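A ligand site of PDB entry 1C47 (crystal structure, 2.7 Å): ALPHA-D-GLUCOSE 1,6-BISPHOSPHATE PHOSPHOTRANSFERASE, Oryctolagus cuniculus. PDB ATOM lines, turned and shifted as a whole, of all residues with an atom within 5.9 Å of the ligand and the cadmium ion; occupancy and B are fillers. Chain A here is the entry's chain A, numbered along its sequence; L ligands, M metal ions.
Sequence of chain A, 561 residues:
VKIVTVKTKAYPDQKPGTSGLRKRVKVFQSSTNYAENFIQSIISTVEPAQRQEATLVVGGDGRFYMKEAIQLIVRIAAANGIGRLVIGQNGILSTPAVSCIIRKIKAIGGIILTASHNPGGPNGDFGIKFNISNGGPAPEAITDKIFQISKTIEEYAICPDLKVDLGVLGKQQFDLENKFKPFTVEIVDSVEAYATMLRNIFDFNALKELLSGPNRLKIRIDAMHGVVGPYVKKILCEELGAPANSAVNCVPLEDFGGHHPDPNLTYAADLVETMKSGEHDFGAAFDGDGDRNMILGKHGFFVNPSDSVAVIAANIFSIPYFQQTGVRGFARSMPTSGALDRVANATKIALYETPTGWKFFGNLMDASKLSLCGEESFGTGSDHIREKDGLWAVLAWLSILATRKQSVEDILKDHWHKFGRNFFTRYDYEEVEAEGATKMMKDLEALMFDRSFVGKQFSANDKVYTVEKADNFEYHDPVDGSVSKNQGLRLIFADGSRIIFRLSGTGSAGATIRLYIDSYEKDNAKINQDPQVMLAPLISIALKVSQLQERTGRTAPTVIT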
ATOM      1  N   THR A  18     -23.601 -17.723 -27.944  1.00  0.00           N
ATOM      2  CA  THR A  18     -22.720 -18.197 -26.801  1.00  0.00           C
ATOM      3  C   THR A  18     -22.366 -19.710 -26.893  1.00  0.00           C
ATOM      4  O   THR A  18     -21.242 -20.114 -26.592  1.00  0.00           O
ATOM      5  CB  THR A  18     -23.420 -17.960 -25.508  1.00  0.00           C
ATOM      6  OG1 THR A  18     -24.745 -18.534 -25.708  1.00  0.00           O
ATOM      7  CG2 THR A  18     -23.494 -16.468 -25.190  1.00  0.00           C
ATOM      8  N   SER A  19     -23.324 -20.550 -27.303  1.00  0.00           N
ATOM      9  CA  SER A  19     -23.027 -21.982 -27.464  1.00  0.00           C
ATOM     10  C   SER A  19     -22.923 -22.361 -28.943  1.00  0.00           C
ATOM     11  O   SER A  19     -23.495 -23.351 -29.414  1.00  0.00           O
ATOM     12  CB  SER A  19     -24.073 -22.853 -26.771  1.00  0.00           C
ATOM     13  OG  SER A  19     -24.023 -22.698 -25.367  1.00  0.00           O
ATOM     14  N   ARG A  22     -26.120 -22.214 -33.532  1.00  0.00           N
ATOM     15  CA  ARG A  22     -27.422 -23.024 -33.598  1.00  0.00           C
ATOM     16  C   ARG A  22     -28.359 -22.444 -34.762  1.00  0.00           C
ATOM     17  O   ARG A  22     -28.596 -21.242 -34.871  1.00  0.00           O
ATOM     18  CB  ARG A  22     -28.158 -22.906 -32.252  1.00  0.00           C
ATOM     19  CG  ARG A  22     -28.272 -24.194 -31.465  1.00  0.00           C
ATOM     20  CD  ARG A  22     -26.855 -24.773 -31.098  1.00  0.00           C
ATOM     21  NE  ARG A  22     -26.392 -24.471 -29.704  1.00  0.00           N
ATOM     22  CZ  ARG A  22     -27.060 -24.955 -28.616  1.00  0.00           C
ATOM     23  NH1 ARG A  22     -28.181 -25.692 -28.749  1.00  0.00           N
ATOM     24  NH2 ARG A  22     -26.565 -24.757 -27.383  1.00  0.00           N
ATOM     25  N   THR A  95     -19.626 -33.650 -26.464  1.00  0.00           N
ATOM     26  CA  THR A  95     -19.009 -32.353 -26.052  1.00  0.00           C
ATOM     27  C   THR A  95     -17.949 -32.500 -24.909  1.00  0.00           C
ATOM     28  O   THR A  95     -16.879 -31.973 -25.027  1.00  0.00           O
ATOM     29  CB  THR A  95     -20.080 -31.364 -25.667  1.00  0.00           C
ATOM     30  OG1 THR A  95     -20.712 -31.039 -26.892  1.00  0.00           O
ATOM     31  CG2 THR A  95     -19.506 -30.078 -25.017  1.00  0.00           C
ATOM     32  N   ALA A 115     -26.214 -29.370 -31.901  1.00  0.00           N
ATOM     33  CA  ALA A 115     -27.202 -28.301 -31.497  1.00  0.00           C
ATOM     34  C   ALA A 115     -27.717 -28.612 -30.076  1.00  0.00           C
ATOM     35  O   ALA A 115     -28.757 -28.120 -29.625  1.00  0.00           O
ATOM     36  CB  ALA A 115     -28.402 -28.303 -32.419  1.00  0.00           C
ATOM     37  N   SER A 116     -26.986 -29.500 -29.360  1.00  0.00           N
ATOM     38  CA  SER A 116     -27.308 -29.825 -27.928  1.00  0.00           C
ATOM     39  C   SER A 116     -28.759 -30.314 -27.623  1.00  0.00           C
ATOM     40  O   SER A 116     -29.249 -31.263 -28.177  1.00  0.00           O
ATOM     41  CB  SER A 116     -26.966 -28.592 -27.015  1.00  0.00           C
ATOM     42  OG  SER A 116     -25.728 -28.742 -26.423  1.00  0.00           O
ATOM     43  N   HIS A 117     -29.455 -29.685 -26.661  1.00  0.00           N
ATOM     44  CA  HIS A 117     -30.871 -30.066 -26.338  1.00  0.00           C
ATOM     45  C   HIS A 117     -31.898 -29.802 -27.544  1.00  0.00           C
ATOM     46  O   HIS A 117     -33.094 -30.089 -27.459  1.00  0.00           O
ATOM     47  CB  HIS A 117     -31.334 -29.273 -25.142  1.00  0.00           C
ATOM     48  CG  HIS A 117     -31.220 -27.766 -25.364  1.00  0.00           C
ATOM     49  ND1 HIS A 117     -30.051 -27.070 -25.283  1.00  0.00           N
ATOM     50  CD2 HIS A 117     -32.236 -26.938 -25.653  1.00  0.00           C
ATOM     51  CE1 HIS A 117     -30.297 -25.782 -25.529  1.00  0.00           C
ATOM     52  NE2 HIS A 117     -31.651 -25.737 -25.731  1.00  0.00           N
ATOM     53  N   LYS A 129     -20.536 -25.711 -33.139  1.00  0.00           N
ATOM     54  CA  LYS A 129     -19.958 -25.130 -31.871  1.00  0.00           C
ATOM     55  C   LYS A 129     -18.349 -25.070 -31.926  1.00  0.00           C
ATOM     56  O   LYS A 129     -17.697 -26.048 -32.169  1.00  0.00           O
ATOM     57  CB  LYS A 129     -20.429 -25.997 -30.701  1.00  0.00           C
ATOM     58  CG  LYS A 129     -19.945 -25.514 -29.362  1.00  0.00           C
ATOM     59  CD  LYS A 129     -21.056 -25.718 -28.296  1.00  0.00           C
ATOM     60  CE  LYS A 129     -21.174 -27.187 -27.870  1.00  0.00           C
ATOM     61  NZ  LYS A 129     -22.281 -27.378 -26.890  1.00  0.00           N
ATOM     62  N   ASP A 287     -28.580 -35.326 -22.617  1.00  0.00           N
ATOM     63  CA  ASP A 287     -29.055 -34.519 -23.779  1.00  0.00           C
ATOM     64  C   ASP A 287     -28.298 -34.826 -25.097  1.00  0.00           C
ATOM     65  O   ASP A 287     -27.458 -35.721 -25.153  1.00  0.00           O
ATOM     66  CB  ASP A 287     -28.937 -33.030 -23.441  1.00  0.00           C
ATOM     67  CG  ASP A 287     -27.514 -32.467 -23.439  1.00  0.00           C
ATOM     68  OD1 ASP A 287     -27.293 -31.316 -23.945  1.00  0.00           O
ATOM     69  OD2 ASP A 287     -26.641 -33.144 -22.942  1.00  0.00           O
ATOM     70  N   GLY A 288     -28.555 -34.049 -26.163  1.00  0.00           N
ATOM     71  CA  GLY A 288     -27.864 -34.257 -27.484  1.00  0.00           C
ATOM     72  C   GLY A 288     -26.316 -34.500 -27.394  1.00  0.00           C
ATOM     73  O   GLY A 288     -25.867 -35.647 -27.450  1.00  0.00           O
ATOM     74  N   ASP A 289     -25.505 -33.452 -27.191  1.00  0.00           N
ATOM     75  CA  ASP A 289     -24.031 -33.648 -27.084  1.00  0.00           C
ATOM     76  C   ASP A 289     -23.561 -34.262 -25.753  1.00  0.00           C
ATOM     77  O   ASP A 289     -22.377 -34.446 -25.513  1.00  0.00           O
ATOM     78  CB  ASP A 289     -23.306 -32.368 -27.349  1.00  0.00           C
ATOM     79  CG  ASP A 289     -23.753 -31.152 -26.521  1.00  0.00           C
ATOM     80  OD1 ASP A 289     -23.391 -30.012 -26.903  1.00  0.00           O
ATOM     81  OD2 ASP A 289     -24.470 -31.320 -25.501  1.00  0.00           O
ATOM     82  N   GLY A 290     -24.450 -34.476 -24.814  1.00  0.00           N
ATOM     83  CA  GLY A 290     -24.050 -35.174 -23.551  1.00  0.00           C
ATOM     84  C   GLY A 290     -23.471 -34.319 -22.382  1.00  0.00           C
ATOM     85  O   GLY A 290     -23.041 -34.860 -21.398  1.00  0.00           O
ATOM     86  N   ASP A 291     -23.537 -33.001 -22.443  1.00  0.00           N
ATOM     87  CA  ASP A 291     -23.039 -32.236 -21.324  1.00  0.00           C
ATOM     88  C   ASP A 291     -24.056 -32.001 -20.189  1.00  0.00           C
ATOM     89  O   ASP A 291     -23.709 -31.401 -19.156  1.00  0.00           O
ATOM     90  CB  ASP A 291     -22.437 -30.912 -21.777  1.00  0.00           C
ATOM     91  CG  ASP A 291     -23.380 -29.864 -22.406  1.00  0.00           C
ATOM     92  OD1 ASP A 291     -24.611 -29.942 -22.202  1.00  0.00           O
ATOM     93  OD2 ASP A 291     -22.858 -28.938 -23.118  1.00  0.00           O
ATOM     94  N   ARG A 292     -25.316 -32.494 -20.351  1.00  0.00           N
ATOM     95  CA  ARG A 292     -26.382 -32.294 -19.309  1.00  0.00           C
ATOM     96  C   ARG A 292     -26.877 -33.579 -18.710  1.00  0.00           C
ATOM     97  O   ARG A 292     -26.650 -34.671 -19.267  1.00  0.00           O
ATOM     98  CB  ARG A 292     -27.540 -31.631 -19.904  1.00  0.00           C
ATOM     99  CG  ARG A 292     -27.327 -30.181 -20.264  1.00  0.00           C
ATOM    100  CD  ARG A 292     -28.685 -29.573 -20.529  1.00  0.00           C
ATOM    101  NE  ARG A 292     -28.590 -28.493 -21.389  1.00  0.00           N
ATOM    102  CZ  ARG A 292     -29.635 -27.757 -21.649  1.00  0.00           C
ATOM    103  NH1 ARG A 292     -30.820 -28.036 -21.094  1.00  0.00           N
ATOM    104  NH2 ARG A 292     -29.506 -26.676 -22.456  1.00  0.00           N
ATOM    105  N   THR A 356     -25.765 -16.810 -16.469  1.00  0.00           N
ATOM    106  CA  THR A 356     -26.078 -18.113 -17.111  1.00  0.00           C
ATOM    107  C   THR A 356     -25.384 -18.163 -18.495  1.00  0.00           C
ATOM    108  O   THR A 356     -25.464 -17.211 -19.296  1.00  0.00           O
ATOM    109  CB  THR A 356     -27.605 -18.351 -17.217  1.00  0.00           C
ATOM    110  OG1 THR A 356     -27.952 -18.860 -18.494  1.00  0.00           O
ATOM    111  CG2 THR A 356     -28.442 -17.099 -16.981  1.00  0.00           C
ATOM    112  N   GLY A 357     -24.714 -19.285 -18.711  1.00  0.00           N
ATOM    113  CA  GLY A 357     -23.915 -19.561 -19.932  1.00  0.00           C
ATOM    114  C   GLY A 357     -22.483 -19.960 -19.527  1.00  0.00           C
ATOM    115  O   GLY A 357     -21.606 -19.109 -19.381  1.00  0.00           O
ATOM    116  N   TRP A 358     -22.307 -21.261 -19.383  1.00  0.00           N
ATOM    117  CA  TRP A 358     -21.065 -21.919 -18.927  1.00  0.00           C
ATOM    118  C   TRP A 358     -19.773 -21.074 -19.071  1.00  0.00           C
ATOM    119  O   TRP A 358     -19.000 -21.022 -18.128  1.00  0.00           O
ATOM    120  CB  TRP A 358     -20.844 -23.226 -19.651  1.00  0.00           C
ATOM    121  CG  TRP A 358     -20.171 -24.219 -18.730  1.00  0.00           C
ATOM    122  CD1 TRP A 358     -20.772 -25.112 -17.938  1.00  0.00           C
ATOM    123  CD2 TRP A 358     -18.787 -24.318 -18.558  1.00  0.00           C
ATOM    124  NE1 TRP A 358     -19.738 -25.795 -17.237  1.00  0.00           N
ATOM    125  CE2 TRP A 358     -18.573 -25.308 -17.610  1.00  0.00           C
ATOM    126  CE3 TRP A 358     -17.686 -23.649 -19.120  1.00  0.00           C
ATOM    127  CZ2 TRP A 358     -17.299 -25.678 -17.168  1.00  0.00           C
ATOM    128  CZ3 TRP A 358     -16.408 -24.041 -18.673  1.00  0.00           C
ATOM    129  CH2 TRP A 358     -16.224 -25.004 -17.743  1.00  0.00           C
ATOM    130  N   GLU A 375     -25.660 -25.416 -13.137  1.00  0.00           N
ATOM    131  CA  GLU A 375     -26.696 -24.511 -13.590  1.00  0.00           C
ATOM    132  C   GLU A 375     -28.039 -25.162 -13.473  1.00  0.00           C
ATOM    133  O   GLU A 375     -28.185 -26.342 -13.728  1.00  0.00           O
ATOM    134  CB  GLU A 375     -26.498 -24.150 -15.072  1.00  0.00           C
ATOM    135  CG  GLU A 375     -25.393 -23.120 -15.319  1.00  0.00           C
ATOM    136  CD  GLU A 375     -25.424 -22.525 -16.708  1.00  0.00           C
ATOM    137  OE1 GLU A 375     -26.345 -21.766 -16.983  1.00  0.00           O
ATOM    138  OE2 GLU A 375     -24.522 -22.781 -17.492  1.00  0.00           O
ATOM    139  N   GLU A 376     -29.067 -24.376 -13.166  1.00  0.00           N
ATOM    140  CA  GLU A 376     -30.421 -24.960 -12.998  1.00  0.00           C
ATOM    141  C   GLU A 376     -30.939 -25.610 -14.327  1.00  0.00           C
ATOM    142  O   GLU A 376     -31.907 -26.338 -14.382  1.00  0.00           O
ATOM    143  CB  GLU A 376     -31.386 -23.897 -12.477  1.00  0.00           C
ATOM    144  CG  GLU A 376     -31.412 -22.621 -13.347  1.00  0.00           C
ATOM    145  CD  GLU A 376     -32.364 -22.716 -14.529  1.00  0.00           C
ATOM    146  OE1 GLU A 376     -33.542 -23.095 -14.298  1.00  0.00           O
ATOM    147  OE2 GLU A 376     -31.924 -22.449 -15.688  1.00  0.00           O
ATOM    148  N   SER A 377     -30.262 -25.362 -15.390  1.00  0.00           N
ATOM    149  CA  SER A 377     -30.608 -25.992 -16.685  1.00  0.00           C
ATOM    150  C   SER A 377     -30.009 -27.413 -16.810  1.00  0.00           C
ATOM    151  O   SER A 377     -29.406 -27.732 -17.808  1.00  0.00           O
ATOM    152  CB  SER A 377     -30.031 -25.171 -17.761  1.00  0.00           C
ATOM    153  OG  SER A 377     -28.666 -24.918 -17.489  1.00  0.00           O
ATOM    154  N   GLU A 387     -15.935 -27.982 -19.997  1.00  0.00           N
ATOM    155  CA  GLU A 387     -17.291 -28.077 -20.494  1.00  0.00           C
ATOM    156  C   GLU A 387     -18.158 -28.757 -19.473  1.00  0.00           C
ATOM    157  O   GLU A 387     -17.655 -29.260 -18.442  1.00  0.00           O
ATOM    158  CB  GLU A 387     -17.328 -28.933 -21.794  1.00  0.00           C
ATOM    159  CG  GLU A 387     -16.939 -28.148 -23.073  1.00  0.00           C
ATOM    160  CD  GLU A 387     -18.029 -27.258 -23.646  1.00  0.00           C
ATOM    161  OE1 GLU A 387     -19.118 -27.133 -23.034  1.00  0.00           O
ATOM    162  OE2 GLU A 387     -17.801 -26.697 -24.727  1.00  0.00           O
ATOM    163  N   LYS A 388     -19.478 -28.785 -19.655  1.00  0.00           N
ATOM    164  CA  LYS A 388     -20.299 -29.543 -18.641  1.00  0.00           C
ATOM    165  C   LYS A 388     -20.130 -31.051 -18.848  1.00  0.00           C
ATOM    166  O   LYS A 388     -19.543 -31.514 -19.850  1.00  0.00           O
ATOM    167  CB  LYS A 388     -21.811 -29.203 -18.744  1.00  0.00           C
ATOM    168  CG  LYS A 388     -22.223 -27.918 -18.044  1.00  0.00           C
ATOM    169  CD  LYS A 388     -23.095 -27.095 -18.984  1.00  0.00           C
ATOM    170  CE  LYS A 388     -24.059 -27.918 -19.555  1.00  0.00           C
ATOM    171  NZ  LYS A 388     -24.659 -27.280 -20.746  1.00  0.00           N
ATOM    172  N   ARG A 502     -36.163 -13.014 -15.312  1.00  0.00           N
ATOM    173  CA  ARG A 502     -35.238 -12.889 -16.431  1.00  0.00           C
ATOM    174  C   ARG A 502     -36.012 -12.734 -17.757  1.00  0.00           C
ATOM    175  O   ARG A 502     -36.395 -13.734 -18.409  1.00  0.00           O
ATOM    176  CB  ARG A 502     -34.351 -14.102 -16.485  1.00  0.00           C
ATOM    177  CG  ARG A 502     -33.037 -13.910 -17.249  1.00  0.00           C
ATOM    178  CD  ARG A 502     -32.039 -14.974 -16.785  1.00  0.00           C
ATOM    179  NE  ARG A 502     -31.019 -15.193 -17.814  1.00  0.00           N
ATOM    180  CZ  ARG A 502     -31.158 -16.190 -18.696  1.00  0.00           C
ATOM    181  NH1 ARG A 502     -32.222 -17.017 -18.644  1.00  0.00           N
ATOM    182  NH2 ARG A 502     -30.198 -16.387 -19.626  1.00  0.00           N
ATOM    183  N   ARG A 514     -38.939 -15.284 -17.932  1.00  0.00           N
ATOM    184  CA  ARG A 514     -38.535 -16.450 -17.124  1.00  0.00           C
ATOM    185  C   ARG A 514     -38.616 -16.178 -15.655  1.00  0.00           C
ATOM    186  O   ARG A 514     -37.814 -15.355 -15.082  1.00  0.00           O
ATOM    187  CB  ARG A 514     -37.164 -16.911 -17.535  1.00  0.00           C
ATOM    188  CG  ARG A 514     -37.307 -17.989 -18.594  1.00  0.00           C
ATOM    189  CD  ARG A 514     -35.972 -18.462 -19.031  1.00  0.00           C
ATOM    190  NE  ARG A 514     -36.128 -19.663 -19.853  1.00  0.00           N
ATOM    191  CZ  ARG A 514     -35.039 -20.236 -20.481  1.00  0.00           C
ATOM    192  NH1 ARG A 514     -33.785 -19.687 -20.333  1.00  0.00           N
ATOM    193  NH2 ARG A 514     -35.207 -21.335 -21.239  1.00  0.00           N
HETATM  194  C1  LIG L   1     -29.418 -21.907 -21.886  1.00  0.00           C
HETATM  195  C2  LIG L   1     -28.916 -22.133 -20.443  1.00  0.00           C
HETATM  196  C3  LIG L   1     -27.376 -22.142 -20.423  1.00  0.00           C
HETATM  197  C4  LIG L   1     -26.752 -23.064 -21.500  1.00  0.00           C
HETATM  198  C5  LIG L   1     -27.331 -22.829 -22.947  1.00  0.00           C
HETATM  199  C6  LIG L   1     -26.784 -23.957 -23.890  1.00  0.00           C
HETATM  200  O1  LIG L   1     -29.057 -20.559 -22.140  1.00  0.00           O
HETATM  201  O2  LIG L   1     -29.353 -21.066 -19.560  1.00  0.00           O
HETATM  202  O3  LIG L   1     -27.077 -22.716 -19.145  1.00  0.00           O
HETATM  203  O4  LIG L   1     -25.412 -22.991 -21.454  1.00  0.00           O
HETATM  204  O5  LIG L   1     -28.789 -22.845 -22.801  1.00  0.00           O
HETATM  205  O6  LIG L   1     -26.750 -25.112 -23.244  1.00  0.00           O
HETATM  206  P1  LIG L   1     -25.666 -26.175 -23.578  1.00  0.00           P
HETATM  207  O7  LIG L   1     -25.546 -26.315 -25.105  1.00  0.00           O
HETATM  208  O8  LIG L   1     -26.095 -27.525 -22.987  1.00  0.00           O
HETATM  209  O9  LIG L   1     -24.325 -25.773 -22.979  1.00  0.00           O
HETATM  210  P2  LIG L   1     -29.928 -19.659 -22.935  1.00  0.00           P
HETATM  211  O10 LIG L   1     -31.364 -20.146 -22.921  1.00  0.00           O
HETATM  212  O11 LIG L   1     -29.847 -18.250 -22.396  1.00  0.00           O
HETATM  213  O12 LIG L   1     -29.454 -19.642 -24.381  1.00  0.00           O
HETATM  214 CD    CD M   1     -25.706 -29.638 -24.322  1.00  0.00          CD
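An oxygen (O3) of the ligand is in hydrogen-bond range of the side-chain carboxylate of Glu 375. NZ of Lys 388 is in salt-bridge range of O9 of the ligand, 2.7 Å away. OG1 of Thr 356 lies within hydrogen-bond range of O2 of the ligand, 2.8 Å away. An oxygen (O7) of the ligand is in salt-bridge range of the guanidinium group (NH2) of Arg 22 (2.9 Å). The guanidinium group of Arg 292 is in hydrogen-bond range of an oxygen (O6) of the ligand. OG of Ser 377 is in hydrogen-bond range of O3 of the ligand. NH2 of Arg 502 lies within salt-bridge range of O11 of the ligand (3.4 Å). The guanidinium group of Arg 514 lies within salt-bridge range of an oxygen (O10) of the ligand, at 3.6 Å. The side-chain amino group (NZ) of Lys 129 lies within salt-bridge range of an oxygen (O7) of the ligand.
N of Arg 292 lies within hydrogen-bond range of OD2 of Asp 287 (3.0 Å). OD1 of Asp 289 lies within salt-bridge range of NZ of Lys 129, 2.9 Å away. OD1 of Asp 289 lies within hydrogen-bond range of OG1 of Thr 95 (2.9 Å). NZ of Lys 388 lies within salt-bridge range of OD2 of Asp 291 (3.4 Å). OE1 of Glu 375 lies within hydrogen-bond range of N of Gly 357, 3.4 Å away. The side-chain carboxylate (OE2) of Glu 375 lies within hydrogen-bond range of the backbone NH (N) of Trp 358, 3.3 Å away. The guanidinium group of Arg 22 lies within hydrogen-bond range of the backbone carbonyl oxygen of Ser 19 (3.1 Å). ND1 of His 117 sits at hydrogen-bond distance from NH2 of Arg 292, 2.9 Å away.
The cadmium ion is bound by OG of Ser 116 (2.3 Å), OD1 of Asp 287 (2.3 Å), OD2 of Asp 289 (2.4 Å), OD1 of Asp 291 (2.4 Å) and O8 of the ligand (2.5 Å).
Within 4 Å of the cadmium ion: Ser 116, Asp 287, Asp 289 and Asp 291. Along chain A the residues within 4 Å of the cadmium ion span positions 116 to 291.
Residues that only touch the ligand: Ser 19 (3.4 Å). Within 4 Å of the ligand: Ser 19, Arg 22, Ser 116, Lys 129, Asp 291, Arg 292, Thr 356, Glu 375, Ser 377, Lys 388, Arg 502 and Arg 514. The nearest printed residue that does not touch the ligand is Gly 357 (4.04 Å).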
